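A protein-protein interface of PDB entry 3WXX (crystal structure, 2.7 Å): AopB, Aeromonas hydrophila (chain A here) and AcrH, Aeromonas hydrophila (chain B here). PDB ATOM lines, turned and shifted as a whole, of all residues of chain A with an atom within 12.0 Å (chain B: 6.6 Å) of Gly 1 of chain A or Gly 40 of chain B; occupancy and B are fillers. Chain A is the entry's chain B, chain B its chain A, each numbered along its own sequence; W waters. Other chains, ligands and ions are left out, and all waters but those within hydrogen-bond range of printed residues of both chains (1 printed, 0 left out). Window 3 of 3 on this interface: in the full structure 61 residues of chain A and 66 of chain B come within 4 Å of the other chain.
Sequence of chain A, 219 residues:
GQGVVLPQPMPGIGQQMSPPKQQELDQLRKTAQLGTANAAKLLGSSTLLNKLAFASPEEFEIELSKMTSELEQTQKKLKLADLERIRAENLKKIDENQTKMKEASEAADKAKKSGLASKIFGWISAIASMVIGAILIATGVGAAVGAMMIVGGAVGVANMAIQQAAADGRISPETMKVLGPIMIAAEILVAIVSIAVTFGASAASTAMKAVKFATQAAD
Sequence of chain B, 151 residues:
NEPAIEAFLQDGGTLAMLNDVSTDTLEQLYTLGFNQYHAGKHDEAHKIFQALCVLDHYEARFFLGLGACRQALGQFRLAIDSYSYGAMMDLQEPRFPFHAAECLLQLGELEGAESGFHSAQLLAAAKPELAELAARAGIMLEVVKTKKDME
Gly 1 of chain A touches Gly 40 of chain B.
Gly 3 of chain A touches Tyr 37 of chain B (N to OH, 3.8 Å).
Val 4 of chain A touches Ala 68 of chain B.
CD1 of Leu 6 of chain A touches CD2 of Tyr 37 of chain B, 3.5 Å away.
Of chain B, only Tyr 37, His 38, Gly 40 and His 42 come within 4 Å of Gly 1 of chain A.
Gly 40 of chain B touches one residue of chain A.
No residue of chain A comes within 4 Å of Gln 36 of chain B.
Of chain A, only Gly 1, Gly 3, Val 4 and Leu 6 come within 4 Å of Tyr 37 of chain B.
His 38 of chain B touches just one residue of chain A: Gly 1.
No residue of chain A comes within 4 Å of Ala 39 of chain B.
No residue of chain A comes within 4 Å of Lys 41 of chain B.
His 42 of chain B touches just one residue of chain A: Gly 1 (3.1 Å).
Printed residues of chain A within 4 Å of Ala 68 of chain B: Val 4.
Of the printed residues of chain B, Leu 6 of chain A touches Tyr 37.
Printed residues of chain B within 4 Å of Gly 3 of chain A: Tyr 37.
Of the printed residues of chain B, Val 4 of chain A touches Tyr 37 and Ala 68.
Gln 2 of chain A touches none of the printed residues of chain B.
The side-chain hydroxyl of Tyr 37 of chain B lies within hydrogen-bond range of the backbone NH of Val 4 of chain A, at 3.0 Å.
The backbone carbonyl oxygen of Tyr 37 of chain B sits at hydrogen-bond distance from the backbone NH of Gly 1 of chain A, 3.1 Å away.
The backbone carbonyl oxygen of Gly 1 of chain A lies within hydrogen-bond range of a ring nitrogen (ND1) of His 38 of chain B, 3.5 Å away.
NE2 of His 42 of chain B lies within hydrogen-bond range of N of Gly 1 of chain A (3.1 Å).
The backbone carbonyl oxygen (O) of Gly 40 of chain B is in hydrogen-bond range of a ring nitrogen (ND1) of His 42 of chain B, at 3.4 Å.
Hydrophobic or aromatic side chains of chain A that line the printed part of chain B: Val 4 and Leu 6.
Of the 11 printed residues of chain B, 5 touch a printed residue of chain A.
Hydrophobic or aromatic side chains of chain B within 4 Å of the printed part of chain A: Tyr 37, His 38, His 42 and Ala 68.
Among the printed residues, no Asp or Glu carboxylate lies within 4 Å of a Lys or Arg side-chain nitrogen of the other chain.
Water W1 lies within hydrogen-bond range of NE2 of His 38 of chain B (2.7 Å) and O of Leu 6 of chain A (3.0 Å).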
ATOM      1  N   GLY A   1       1.405  -5.440  24.645  1.00  0.00           N
ATOM      2  CA  GLY A   1       1.182  -5.960  23.269  1.00  0.00           C
ATOM      3  C   GLY A   1       2.447  -6.603  22.754  1.00  0.00           C
ATOM      4  O   GLY A   1       3.400  -5.909  22.414  1.00  0.00           O
ATOM      5  N   GLN A   2       2.459  -7.932  22.737  1.00  0.00           N
ATOM      6  CA  GLN A   2       3.589  -8.718  22.240  1.00  0.00           C
ATOM      7  C   GLN A   2       3.303  -9.277  20.838  1.00  0.00           C
ATOM      8  O   GLN A   2       4.124 -10.018  20.276  1.00  0.00           O
ATOM      9  CB  GLN A   2       3.896  -9.897  23.195  1.00  0.00           C
ATOM     10  CG  GLN A   2       3.885  -9.620  24.700  1.00  0.00           C
ATOM     11  CD  GLN A   2       4.775 -10.578  25.496  1.00  0.00           C
ATOM     12  OE1 GLN A   2       5.381 -11.504  24.948  1.00  0.00           O
ATOM     13  NE2 GLN A   2       4.854 -10.353  26.801  1.00  0.00           N
ATOM     14  N   GLY A   3       2.148  -8.920  20.274  1.00  0.00           N
ATOM     15  CA  GLY A   3       1.749  -9.393  18.947  1.00  0.00           C
ATOM     16  C   GLY A   3       2.556  -8.775  17.806  1.00  0.00           C
ATOM     17  O   GLY A   3       3.001  -9.487  16.908  1.00  0.00           O
ATOM     18  N   VAL A   4       2.754  -7.455  17.829  1.00  0.00           N
ATOM     19  CA  VAL A   4       3.444  -6.780  16.728  1.00  0.00           C
ATOM     20  C   VAL A   4       4.786  -6.195  17.136  1.00  0.00           C
ATOM     21  O   VAL A   4       4.913  -5.528  18.178  1.00  0.00           O
ATOM     22  CB  VAL A   4       2.571  -5.697  16.035  1.00  0.00           C
ATOM     23  CG1 VAL A   4       3.245  -5.188  14.770  1.00  0.00           C
ATOM     24  CG2 VAL A   4       1.207  -6.271  15.678  1.00  0.00           C
ATOM     25  N   VAL A   5       5.788  -6.474  16.298  1.00  0.00           N
ATOM     26  CA  VAL A   5       7.108  -5.894  16.439  1.00  0.00           C
ATOM     27  C   VAL A   5       7.095  -4.552  15.750  1.00  0.00           C
ATOM     28  O   VAL A   5       7.114  -4.479  14.525  1.00  0.00           O
ATOM     29  CB  VAL A   5       8.200  -6.760  15.760  1.00  0.00           C
ATOM     30  CG1 VAL A   5       9.512  -6.011  15.686  1.00  0.00           C
ATOM     31  CG2 VAL A   5       8.384  -8.076  16.485  1.00  0.00           C
ATOM     32  N   LEU A   6       7.075  -3.488  16.534  1.00  0.00           N
ATOM     33  CA  LEU A   6       7.198  -2.151  15.979  1.00  0.00           C
ATOM     34  C   LEU A   6       8.672  -1.804  15.880  1.00  0.00           C
ATOM     35  O   LEU A   6       9.458  -2.208  16.752  1.00  0.00           O
ATOM     36  CB  LEU A   6       6.546  -1.147  16.914  1.00  0.00           C
ATOM     37  CG  LEU A   6       5.134  -1.458  17.342  1.00  0.00           C
ATOM     38  CD1 LEU A   6       4.711  -0.401  18.335  1.00  0.00           C
ATOM     39  CD2 LEU A   6       4.216  -1.456  16.132  1.00  0.00           C
ATOM     40  N   PRO A   7       9.065  -1.009  14.863  1.00  0.00           N
ATOM     41  CA  PRO A   7      10.472  -0.582  14.823  1.00  0.00           C
ATOM     42  C   PRO A   7      10.845   0.227  16.023  1.00  0.00           C
ATOM     43  O   PRO A   7       9.996   0.926  16.574  1.00  0.00           O
ATOM     44  CB  PRO A   7      10.560   0.258  13.544  1.00  0.00           C
ATOM     45  CG  PRO A   7       9.167   0.539  13.139  1.00  0.00           C
ATOM     46  CD  PRO A   7       8.367  -0.633  13.624  1.00  0.00           C
ATOM     47  N   GLN A   8      12.112   0.138  16.413  1.00  0.00           N
ATOM     48  CA  GLN A   8      12.604   0.820  17.623  1.00  0.00           C
ATOM     49  C   GLN A   8      12.699   2.307  17.418  1.00  0.00           C
ATOM     50  O   GLN A   8      13.019   2.742  16.326  1.00  0.00           O
ATOM     51  CB  GLN A   8      13.976   0.306  18.035  1.00  0.00           C
ATOM     52  CG  GLN A   8      13.927  -1.101  18.608  1.00  0.00           C
ATOM     53  CD  GLN A   8      13.655  -1.101  20.116  1.00  0.00           C
ATOM     54  OE1 GLN A   8      12.933  -1.962  20.606  1.00  0.00           O
ATOM     55  NE2 GLN A   8      14.179  -0.093  20.850  1.00  0.00           N
ATOM     56  N   ASN B  35       6.451   2.778  23.798  1.00  0.00           N
ATOM     57  CA  ASN B  35       6.557   2.251  25.157  1.00  0.00           C
ATOM     58  C   ASN B  35       5.173   1.890  25.683  1.00  0.00           C
ATOM     59  O   ASN B  35       4.971   0.795  26.221  1.00  0.00           O
ATOM     60  CB  ASN B  35       7.206   3.234  26.116  1.00  0.00           C
ATOM     61  CG  ASN B  35       8.630   3.523  25.761  1.00  0.00           C
ATOM     62  OD1 ASN B  35       9.310   2.706  25.185  1.00  0.00           O
ATOM     63  ND2 ASN B  35       9.054   4.756  26.007  1.00  0.00           N
ATOM     64  N   GLN B  36       4.221   2.802  25.535  1.00  0.00           N
ATOM     65  CA  GLN B  36       2.884   2.517  26.010  1.00  0.00           C
ATOM     66  C   GLN B  36       2.310   1.219  25.431  1.00  0.00           C
ATOM     67  O   GLN B  36       1.607   0.468  26.111  1.00  0.00           O
ATOM     68  CB  GLN B  36       1.956   3.693  25.711  1.00  0.00           C
ATOM     69  CG  GLN B  36       2.317   4.954  26.477  1.00  0.00           C
ATOM     70  CD  GLN B  36       2.086   4.787  27.967  1.00  0.00           C
ATOM     71  OE1 GLN B  36       2.764   3.983  28.619  1.00  0.00           O
ATOM     72  NE2 GLN B  36       1.117   5.520  28.508  1.00  0.00           N
ATOM     73  N   TYR B  37       2.590   0.969  24.153  1.00  0.00           N
ATOM     74  CA  TYR B  37       2.074  -0.232  23.521  1.00  0.00           C
ATOM     75  C   TYR B  37       2.704  -1.424  24.211  1.00  0.00           C
ATOM     76  O   TYR B  37       2.004  -2.367  24.571  1.00  0.00           O
ATOM     77  CB  TYR B  37       2.365  -0.231  22.018  1.00  0.00           C
ATOM     78  CG  TYR B  37       2.181  -1.553  21.335  1.00  0.00           C
ATOM     79  CD1 TYR B  37       0.924  -2.045  21.089  1.00  0.00           C
ATOM     80  CD2 TYR B  37       3.265  -2.318  20.942  1.00  0.00           C
ATOM     81  CE1 TYR B  37       0.732  -3.259  20.478  1.00  0.00           C
ATOM     82  CE2 TYR B  37       3.079  -3.547  20.316  1.00  0.00           C
ATOM     83  CZ  TYR B  37       1.811  -4.013  20.078  1.00  0.00           C
ATOM     84  OH  TYR B  37       1.598  -5.224  19.435  1.00  0.00           O
ATOM     85  N   HIS B  38       4.022  -1.390  24.403  1.00  0.00           N
ATOM     86  CA  HIS B  38       4.715  -2.519  25.032  1.00  0.00           C
ATOM     87  C   HIS B  38       4.364  -2.640  26.537  1.00  0.00           C
ATOM     88  O   HIS B  38       4.439  -3.727  27.113  1.00  0.00           O
ATOM     89  CB  HIS B  38       6.221  -2.452  24.761  1.00  0.00           C
ATOM     90  CG  HIS B  38       6.602  -2.892  23.384  1.00  0.00           C
ATOM     91  ND1 HIS B  38       6.351  -4.161  22.921  1.00  0.00           N
ATOM     92  CD2 HIS B  38       7.232  -2.243  22.372  1.00  0.00           C
ATOM     93  CE1 HIS B  38       6.801  -4.278  21.679  1.00  0.00           C
ATOM     94  NE2 HIS B  38       7.331  -3.125  21.318  1.00  0.00           N
ATOM     95  N   ALA B  39       3.941  -1.546  27.155  1.00  0.00           N
ATOM     96  CA  ALA B  39       3.397  -1.593  28.515  1.00  0.00           C
ATOM     97  C   ALA B  39       1.985  -2.171  28.606  1.00  0.00           C
ATOM     98  O   ALA B  39       1.436  -2.298  29.705  1.00  0.00           O
ATOM     99  CB  ALA B  39       3.401  -0.196  29.131  1.00  0.00           C
ATOM    100  N   GLY B  40       1.396  -2.538  27.477  1.00  0.00           N
ATOM    101  CA  GLY B  40       0.011  -3.013  27.441  1.00  0.00           C
ATOM    102  C   GLY B  40      -1.038  -1.919  27.588  1.00  0.00           C
ATOM    103  O   GLY B  40      -2.226  -2.225  27.632  1.00  0.00           O
ATOM    104  N   LYS B  41      -0.622  -0.655  27.698  1.00  0.00           N
ATOM    105  CA  LYS B  41      -1.565   0.465  27.752  1.00  0.00           C
ATOM    106  C   LYS B  41      -2.116   0.779  26.360  1.00  0.00           C
ATOM    107  O   LYS B  41      -1.957   1.883  25.839  1.00  0.00           O
ATOM    108  CB  LYS B  41      -0.888   1.717  28.320  1.00  0.00           C
ATOM    109  CG  LYS B  41      -0.329   1.612  29.728  1.00  0.00           C
ATOM    110  CD  LYS B  41      -1.394   1.325  30.775  1.00  0.00           C
ATOM    111  CE  LYS B  41      -0.754   1.072  32.137  1.00  0.00           C
ATOM    112  NZ  LYS B  41      -0.742   2.282  33.023  1.00  0.00           N
ATOM    113  N   HIS B  42      -2.797  -0.187  25.777  1.00  0.00           N
ATOM    114  CA  HIS B  42      -3.125  -0.175  24.352  1.00  0.00           C
ATOM    115  C   HIS B  42      -4.028   0.940  23.926  1.00  0.00           C
ATOM    116  O   HIS B  42      -3.857   1.521  22.845  1.00  0.00           O
ATOM    117  CB  HIS B  42      -3.800  -1.467  23.976  1.00  0.00           C
ATOM    118  CG  HIS B  42      -2.936  -2.648  24.182  1.00  0.00           C
ATOM    119  ND1 HIS B  42      -3.365  -3.770  24.845  1.00  0.00           N
ATOM    120  CD2 HIS B  42      -1.651  -2.876  23.846  1.00  0.00           C
ATOM    121  CE1 HIS B  42      -2.388  -4.659  24.874  1.00  0.00           C
ATOM    122  NE2 HIS B  42      -1.333  -4.135  24.285  1.00  0.00           N
ATOM    123  N   ASP B  43      -4.990   1.244  24.780  1.00  0.00           N
ATOM    124  CA  ASP B  43      -5.931   2.304  24.506  1.00  0.00           C
ATOM    125  C   ASP B  43      -5.227   3.667  24.441  1.00  0.00           C
ATOM    126  O   ASP B  43      -5.488   4.469  23.554  1.00  0.00           O
ATOM    127  CB  ASP B  43      -7.002   2.309  25.588  1.00  0.00           C
ATOM    128  CG  ASP B  43      -8.232   2.970  25.143  1.00  0.00           C
ATOM    129  OD1 ASP B  43      -9.022   2.291  24.445  1.00  0.00           O
ATOM    130  OD2 ASP B  43      -8.363   4.177  25.461  1.00  0.00           O
ATOM    131  N   ALA B  68      -1.439  -2.115  15.370  1.00  0.00           N
ATOM    132  CA  ALA B  68      -1.111  -3.003  16.451  1.00  0.00           C
ATOM    133  C   ALA B  68      -1.947  -2.676  17.700  1.00  0.00           C
ATOM    134  O   ALA B  68      -2.404  -3.584  18.359  1.00  0.00           O
ATOM    135  CB  ALA B  68       0.359  -2.916  16.755  1.00  0.00           C
ATOM    136  N   ALA B  72      -4.622  -5.471  19.366  1.00  0.00           N
ATOM    137  CA  ALA B  72      -4.602  -5.802  20.778  1.00  0.00           C
ATOM    138  C   ALA B  72      -5.922  -5.513  21.494  1.00  0.00           C
ATOM    139  O   ALA B  72      -6.308  -6.295  22.339  1.00  0.00           O
ATOM    140  CB  ALA B  72      -3.488  -5.051  21.496  1.00  0.00           C
HETATM  141  O   HOH W   1       8.625  -3.905  19.140  1.00  0.00           O
